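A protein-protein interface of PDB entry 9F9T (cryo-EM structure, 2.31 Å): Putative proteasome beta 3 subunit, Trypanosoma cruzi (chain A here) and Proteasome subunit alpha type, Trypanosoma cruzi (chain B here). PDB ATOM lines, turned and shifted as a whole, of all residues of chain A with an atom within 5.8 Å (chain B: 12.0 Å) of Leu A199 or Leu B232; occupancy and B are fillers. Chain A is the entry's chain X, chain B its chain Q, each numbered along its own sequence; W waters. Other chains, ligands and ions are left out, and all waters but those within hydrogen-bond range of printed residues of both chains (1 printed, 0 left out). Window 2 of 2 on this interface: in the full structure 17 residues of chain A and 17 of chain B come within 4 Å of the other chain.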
ATOM      1  N   ASN A  26     -36.002 -21.491  -4.916  1.00  0.00           N
ATOM      2  CA  ASN A  26     -35.403 -22.439  -3.947  1.00  0.00           C
ATOM      3  C   ASN A  26     -36.395 -23.468  -3.407  1.00  0.00           C
ATOM      4  O   ASN A  26     -36.084 -24.268  -2.555  1.00  0.00           O
ATOM      5  CB  ASN A  26     -34.972 -21.751  -2.668  1.00  0.00           C
ATOM      6  CG  ASN A  26     -33.691 -20.987  -2.778  1.00  0.00           C
ATOM      7  OD1 ASN A  26     -32.659 -21.509  -3.194  1.00  0.00           O
ATOM      8  ND2 ASN A  26     -33.775 -19.710  -2.497  1.00  0.00           N
ATOM      9  N   PRO A  40     -31.997 -25.012  -4.533  1.00  0.00           N
ATOM     10  CA  PRO A  40     -31.742 -24.378  -5.818  1.00  0.00           C
ATOM     11  C   PRO A  40     -31.462 -25.404  -6.916  1.00  0.00           C
ATOM     12  O   PRO A  40     -31.047 -26.542  -6.639  1.00  0.00           O
ATOM     13  CB  PRO A  40     -30.522 -23.498  -5.574  1.00  0.00           C
ATOM     14  CG  PRO A  40     -29.868 -24.057  -4.326  1.00  0.00           C
ATOM     15  CD  PRO A  40     -30.851 -24.978  -3.649  1.00  0.00           C
ATOM     16  N   GLY A 184     -37.293 -17.143  -2.393  1.00  0.00           N
ATOM     17  CA  GLY A 184     -36.104 -16.391  -2.759  1.00  0.00           C
ATOM     18  C   GLY A 184     -35.300 -17.124  -3.818  1.00  0.00           C
ATOM     19  O   GLY A 184     -35.863 -18.007  -4.445  1.00  0.00           O
ATOM     20  N   ALA A 185     -34.038 -16.776  -4.039  1.00  0.00           N
ATOM     21  CA  ALA A 185     -33.377 -17.281  -5.225  1.00  0.00           C
ATOM     22  C   ALA A 185     -31.888 -17.303  -5.090  1.00  0.00           C
ATOM     23  O   ALA A 185     -31.311 -16.718  -4.198  1.00  0.00           O
ATOM     24  CB  ALA A 185     -33.704 -16.411  -6.379  1.00  0.00           C
ATOM     25  N   VAL A 186     -31.302 -18.064  -5.966  1.00  0.00           N
ATOM     26  CA  VAL A 186     -29.867 -18.143  -6.121  1.00  0.00           C
ATOM     27  C   VAL A 186     -29.524 -17.752  -7.565  1.00  0.00           C
ATOM     28  O   VAL A 186     -30.285 -18.042  -8.473  1.00  0.00           O
ATOM     29  CB  VAL A 186     -29.386 -19.566  -5.828  1.00  0.00           C
ATOM     30  CG1 VAL A 186     -27.897 -19.527  -5.807  1.00  0.00           C
ATOM     31  CG2 VAL A 186     -29.783 -20.059  -4.474  1.00  0.00           C
ATOM     32  N   ALA A 187     -28.449 -17.008  -7.729  1.00  0.00           N
ATOM     33  CA  ALA A 187     -28.046 -16.477  -9.016  1.00  0.00           C
ATOM     34  C   ALA A 187     -26.575 -16.705  -9.173  1.00  0.00           C
ATOM     35  O   ALA A 187     -25.808 -16.430  -8.260  1.00  0.00           O
ATOM     36  CB  ALA A 187     -28.299 -14.993  -9.168  1.00  0.00           C
ATOM     37  N   THR A 197     -21.842 -15.704  -7.078  1.00  0.00           N
ATOM     38  CA  THR A 197     -23.090 -16.344  -6.731  1.00  0.00           C
ATOM     39  C   THR A 197     -23.796 -15.508  -5.712  1.00  0.00           C
ATOM     40  O   THR A 197     -23.180 -14.909  -4.869  1.00  0.00           O
ATOM     41  CB  THR A 197     -22.850 -17.756  -6.214  1.00  0.00           C
ATOM     42  OG1 THR A 197     -22.314 -18.578  -7.250  1.00  0.00           O
ATOM     43  CG2 THR A 197     -24.158 -18.386  -5.798  1.00  0.00           C
ATOM     44  N   ARG A 198     -25.089 -15.423  -5.757  1.00  0.00           N
ATOM     45  CA  ARG A 198     -25.735 -14.589  -4.768  1.00  0.00           C
ATOM     46  C   ARG A 198     -27.039 -15.215  -4.334  1.00  0.00           C
ATOM     47  O   ARG A 198     -27.824 -15.659  -5.165  1.00  0.00           O
ATOM     48  CB  ARG A 198     -26.101 -13.233  -5.379  1.00  0.00           C
ATOM     49  CG  ARG A 198     -24.889 -12.397  -5.740  1.00  0.00           C
ATOM     50  CD  ARG A 198     -25.248 -10.982  -6.038  1.00  0.00           C
ATOM     51  NE  ARG A 198     -24.006 -10.262  -6.237  1.00  0.00           N
ATOM     52  CZ  ARG A 198     -23.834  -9.307  -7.131  1.00  0.00           C
ATOM     53  NH1 ARG A 198     -24.828  -8.961  -7.932  1.00  0.00           N
ATOM     54  NH2 ARG A 198     -22.659  -8.719  -7.227  1.00  0.00           N
ATOM     55  N   LEU A 199     -27.279 -15.208  -3.054  1.00  0.00           N
ATOM     56  CA  LEU A 199     -28.561 -15.661  -2.560  1.00  0.00           C
ATOM     57  C   LEU A 199     -29.408 -14.417  -2.330  1.00  0.00           C
ATOM     58  O   LEU A 199     -29.021 -13.551  -1.604  1.00  0.00           O
ATOM     59  CB  LEU A 199     -28.310 -16.465  -1.272  1.00  0.00           C
ATOM     60  CG  LEU A 199     -29.560 -16.833  -0.467  1.00  0.00           C
ATOM     61  CD1 LEU A 199     -30.380 -17.913  -1.169  1.00  0.00           C
ATOM     62  CD2 LEU A 199     -29.230 -17.283   0.957  1.00  0.00           C
ATOM     63  N   ILE A 200     -30.543 -14.325  -2.996  1.00  0.00           N
ATOM     64  CA  ILE A 200     -31.426 -13.169  -2.978  1.00  0.00           C
ATOM     65  C   ILE A 200     -32.566 -13.405  -2.008  1.00  0.00           C
ATOM     66  O   ILE A 200     -33.158 -14.457  -2.049  1.00  0.00           O
ATOM     67  CB  ILE A 200     -32.024 -13.038  -4.384  1.00  0.00           C
ATOM     68  CG1 ILE A 200     -30.917 -12.968  -5.428  1.00  0.00           C
ATOM     69  CG2 ILE A 200     -33.020 -11.893  -4.495  1.00  0.00           C
ATOM     70  CD1 ILE A 200     -31.491 -13.056  -6.833  1.00  0.00           C
ATOM     71  N   ASN A 201     -32.936 -12.422  -1.212  1.00  0.00           N
ATOM     72  CA  ASN A 201     -34.069 -12.590  -0.310  1.00  0.00           C
ATOM     73  C   ASN A 201     -35.403 -12.587  -1.071  1.00  0.00           C
ATOM     74  O   ASN A 201     -35.531 -11.923  -2.084  1.00  0.00           O
ATOM     75  CB  ASN A 201     -34.109 -11.483   0.739  1.00  0.00           C
ATOM     76  CG  ASN A 201     -34.743 -11.950   2.028  1.00  0.00           C
ATOM     77  OD1 ASN A 201     -34.526 -13.084   2.453  1.00  0.00           O
ATOM     78  ND2 ASN A 201     -35.519 -11.083   2.662  1.00  0.00           N
ATOM     79  N   PRO B 227     -10.795 -26.710  -3.449  1.00  0.00           N
ATOM     80  CA  PRO B 227     -11.238 -25.474  -4.092  1.00  0.00           C
ATOM     81  C   PRO B 227     -12.470 -24.865  -3.409  1.00  0.00           C
ATOM     82  O   PRO B 227     -12.885 -25.309  -2.336  1.00  0.00           O
ATOM     83  CB  PRO B 227     -11.504 -25.949  -5.535  1.00  0.00           C
ATOM     84  CG  PRO B 227     -11.988 -27.366  -5.370  1.00  0.00           C
ATOM     85  CD  PRO B 227     -11.119 -27.902  -4.253  1.00  0.00           C
ATOM     86  N   ALA B 228     -13.024 -23.827  -4.054  1.00  0.00           N
ATOM     87  CA  ALA B 228     -14.258 -23.158  -3.659  1.00  0.00           C
ATOM     88  C   ALA B 228     -15.228 -24.106  -2.953  1.00  0.00           C
ATOM     89  O   ALA B 228     -15.398 -25.256  -3.357  1.00  0.00           O
ATOM     90  CB  ALA B 228     -14.913 -22.563  -4.888  1.00  0.00           C
ATOM     91  N   THR B 229     -15.881 -23.587  -1.909  1.00  0.00           N
ATOM     92  CA  THR B 229     -17.041 -24.224  -1.305  1.00  0.00           C
ATOM     93  C   THR B 229     -18.287 -23.452  -1.743  1.00  0.00           C
ATOM     94  O   THR B 229     -18.514 -22.340  -1.262  1.00  0.00           O
ATOM     95  CB  THR B 229     -16.874 -24.308   0.221  1.00  0.00           C
ATOM     96  OG1 THR B 229     -16.119 -23.178   0.665  1.00  0.00           O
ATOM     97  CG2 THR B 229     -16.170 -25.570   0.670  1.00  0.00           C
ATOM     98  N   GLN B 230     -19.067 -24.043  -2.669  1.00  0.00           N
ATOM     99  CA  GLN B 230     -20.259 -23.412  -3.228  1.00  0.00           C
ATOM    100  C   GLN B 230     -21.462 -23.648  -2.325  1.00  0.00           C
ATOM    101  O   GLN B 230     -22.348 -24.395  -2.689  1.00  0.00           O
ATOM    102  CB  GLN B 230     -20.640 -23.995  -4.595  1.00  0.00           C
ATOM    103  CG  GLN B 230     -19.632 -23.760  -5.711  1.00  0.00           C
ATOM    104  CD  GLN B 230     -19.922 -24.640  -6.910  1.00  0.00           C
ATOM    105  OE1 GLN B 230     -20.146 -25.844  -6.792  1.00  0.00           O
ATOM    106  NE2 GLN B 230     -19.912 -24.046  -8.092  1.00  0.00           N
ATOM    107  N   LYS B 231     -21.506 -22.994  -1.169  1.00  0.00           N
ATOM    108  CA  LYS B 231     -22.541 -23.253  -0.183  1.00  0.00           C
ATOM    109  C   LYS B 231     -23.900 -22.698  -0.616  1.00  0.00           C
ATOM    110  O   LYS B 231     -24.891 -22.950   0.066  1.00  0.00           O
ATOM    111  CB  LYS B 231     -22.134 -22.671   1.181  1.00  0.00           C
ATOM    112  CG  LYS B 231     -21.386 -23.632   2.096  1.00  0.00           C
ATOM    113  CD  LYS B 231     -20.577 -22.931   3.166  1.00  0.00           C
ATOM    114  CE  LYS B 231     -19.474 -23.802   3.731  1.00  0.00           C
ATOM    115  NZ  LYS B 231     -18.291 -22.999   4.125  1.00  0.00           N
ATOM    116  N   LEU B 232     -23.950 -21.882  -1.681  1.00  0.00           N
ATOM    117  CA  LEU B 232     -25.213 -21.304  -2.119  1.00  0.00           C
ATOM    118  C   LEU B 232     -25.889 -22.241  -3.101  1.00  0.00           C
ATOM    119  O   LEU B 232     -27.097 -22.409  -2.988  1.00  0.00           O
ATOM    120  CB  LEU B 232     -24.983 -19.918  -2.733  1.00  0.00           C
ATOM    121  CG  LEU B 232     -24.214 -18.986  -1.806  1.00  0.00           C
ATOM    122  CD1 LEU B 232     -24.260 -17.545  -2.290  1.00  0.00           C
ATOM    123  CD2 LEU B 232     -24.753 -19.111  -0.376  1.00  0.00           C
ATOM    124  N   LEU B 233     -25.117 -22.839  -4.024  1.00  0.00           N
ATOM    125  CA  LEU B 233     -25.665 -23.812  -4.970  1.00  0.00           C
ATOM    126  C   LEU B 233     -25.834 -25.196  -4.328  1.00  0.00           C
ATOM    127  O   LEU B 233     -26.587 -26.006  -4.856  1.00  0.00           O
ATOM    128  CB  LEU B 233     -24.808 -23.916  -6.245  1.00  0.00           C
ATOM    129  CG  LEU B 233     -24.659 -22.656  -7.112  1.00  0.00           C
ATOM    130  CD1 LEU B 233     -24.327 -23.030  -8.542  1.00  0.00           C
ATOM    131  CD2 LEU B 233     -25.895 -21.765  -7.092  1.00  0.00           C
ATOM    132  N   GLU B 234     -25.215 -25.466  -3.179  1.00  0.00           N
ATOM    133  CA  GLU B 234     -25.328 -26.762  -2.501  1.00  0.00           C
ATOM    134  C   GLU B 234     -25.277 -26.541  -1.001  1.00  0.00           C
ATOM    135  O   GLU B 234     -24.195 -26.590  -0.430  1.00  0.00           O
ATOM    136  CB  GLU B 234     -24.143 -27.709  -2.725  1.00  0.00           C
ATOM    137  CG  GLU B 234     -24.249 -28.586  -3.945  1.00  0.00           C
ATOM    138  CD  GLU B 234     -23.510 -28.062  -5.158  1.00  0.00           C
ATOM    139  OE1 GLU B 234     -22.258 -28.245  -5.225  1.00  0.00           O
ATOM    140  OE2 GLU B 234     -24.192 -27.476  -6.034  1.00  0.00           O
ATOM    141  N   PRO B 235     -26.399 -26.245  -0.320  1.00  0.00           N
ATOM    142  CA  PRO B 235     -26.313 -25.922   1.101  1.00  0.00           C
ATOM    143  C   PRO B 235     -25.986 -27.109   1.999  1.00  0.00           C
ATOM    144  O   PRO B 235     -25.684 -26.943   3.172  1.00  0.00           O
ATOM    145  CB  PRO B 235     -27.662 -25.239   1.407  1.00  0.00           C
ATOM    146  CG  PRO B 235     -28.318 -24.997   0.025  1.00  0.00           C
ATOM    147  CD  PRO B 235     -27.735 -26.040  -0.903  1.00  0.00           C
ATOM    148  N   TYR B 236     -26.043 -28.312   1.474  1.00  0.00           N
ATOM    149  CA  TYR B 236     -25.677 -29.479   2.269  1.00  0.00           C
ATOM    150  C   TYR B 236     -24.477 -30.157   1.596  1.00  0.00           C
ATOM    151  O   TYR B 236     -24.252 -31.344   1.765  1.00  0.00           O
ATOM    152  CB  TYR B 236     -26.881 -30.426   2.454  1.00  0.00           C
ATOM    153  CG  TYR B 236     -28.078 -29.947   3.269  1.00  0.00           C
ATOM    154  CD1 TYR B 236     -28.123 -30.034   4.659  1.00  0.00           C
ATOM    155  CD2 TYR B 236     -29.183 -29.401   2.640  1.00  0.00           C
ATOM    156  CE1 TYR B 236     -29.238 -29.623   5.392  1.00  0.00           C
ATOM    157  CE2 TYR B 236     -30.287 -28.959   3.354  1.00  0.00           C
ATOM    158  CZ  TYR B 236     -30.323 -29.059   4.735  1.00  0.00           C
ATOM    159  OH  TYR B 236     -31.465 -28.594   5.348  1.00  0.00           O
ATOM    160  N   GLY B 237     -23.719 -29.408   0.807  1.00  0.00           N
ATOM    161  CA  GLY B 237     -22.394 -29.849   0.399  1.00  0.00           C
ATOM    162  C   GLY B 237     -21.382 -29.727   1.545  1.00  0.00           C
ATOM    163  O   GLY B 237     -21.400 -28.763   2.311  1.00  0.00           O
ATOM    164  N   VAL B 238     -20.501 -30.723   1.666  1.00  0.00           N
ATOM    165  CA  VAL B 238     -19.390 -30.626   2.599  1.00  0.00           C
ATOM    166  C   VAL B 238     -18.155 -31.180   1.895  1.00  0.00           C
ATOM    167  O   VAL B 238     -18.157 -32.322   1.430  1.00  0.00           O
ATOM    168  CB  VAL B 238     -19.672 -31.337   3.942  1.00  0.00           C
ATOM    169  CG1 VAL B 238     -18.670 -30.929   5.023  1.00  0.00           C
ATOM    170  CG2 VAL B 238     -21.097 -31.100   4.431  1.00  0.00           C
ATOM    171  N   LEU B 239     -17.122 -30.335   1.799  1.00  0.00           N
ATOM    172  CA  LEU B 239     -15.849 -30.757   1.245  1.00  0.00           C
ATOM    173  C   LEU B 239     -14.824 -30.843   2.370  1.00  0.00           C
ATOM    174  O   LEU B 239     -14.877 -30.119   3.365  1.00  0.00           O
ATOM    175  CB  LEU B 239     -15.387 -29.792   0.145  1.00  0.00           C
ATOM    176  CG  LEU B 239     -16.024 -29.948  -1.242  1.00  0.00           C
ATOM    177  CD1 LEU B 239     -15.287 -29.078  -2.257  1.00  0.00           C
ATOM    178  CD2 LEU B 239     -16.045 -31.404  -1.706  1.00  0.00           C
HETATM  179  O   HOH W   1     -28.032 -24.923  -7.134  1.00  0.00           O
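Among the printed residues, pairs that only touch across the chains: Val A186 with Leu B233 (3.3 Å), Pro A40 with Leu B232 (3.5 Å), Thr A197 with Leu B232 (3.5 Å), Pro A40 with Leu B233 (3.9 Å), Val A186 with Leu B232 (3.9 Å) and Leu A199 with Leu B232 (3.9 Å).
Pro A40 touches just these residues of chain B: Leu B232 (3.5 Å) and Leu B233 (3.9 Å).
No residue of chain B comes within 4 Å of Gly A184.
Ala A185 touches none of the printed residues of chain B.
Of chain B, only Leu B232 (3.9 Å) and Leu B233 (3.3 Å) come within 4 Å of Val A186.
Printed residues of chain B within 4 Å of Thr A197: Leu B232 (3.5 Å).
Leu A199 touches one residue of chain B.
Gln B230 touches none of the printed residues of chain A.
Printed residues of chain A within 4 Å of Leu B233: Pro A40 (3.9 Å) and Val A186 (3.3 Å).
The nearest residue of chain A that does not touch Leu B232 is Arg A198 (4.1 Å).
Printed residues of chain A that touch a printed residue of chain B: Pro A40, Val A186, Thr A197 and Leu A199.
Hydrophobic or aromatic side chains of chain A that line the printed part of chain B: Pro A40 and Val A186.
Hydrophobic or aromatic side chains of chain B within 4 Å of the printed part of chain A: Leu B232 and Leu B233.
Among the printed residues, no Asp or Glu carboxylate lies within 4 Å of a Lys or Arg side-chain nitrogen of the other chain.
Water W1 bridges the backbone carbonyl oxygen (O) of Leu B233 (2.9 Å) and the backbone carbonyl oxygen (O) of Pro A40 (3.5 Å).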
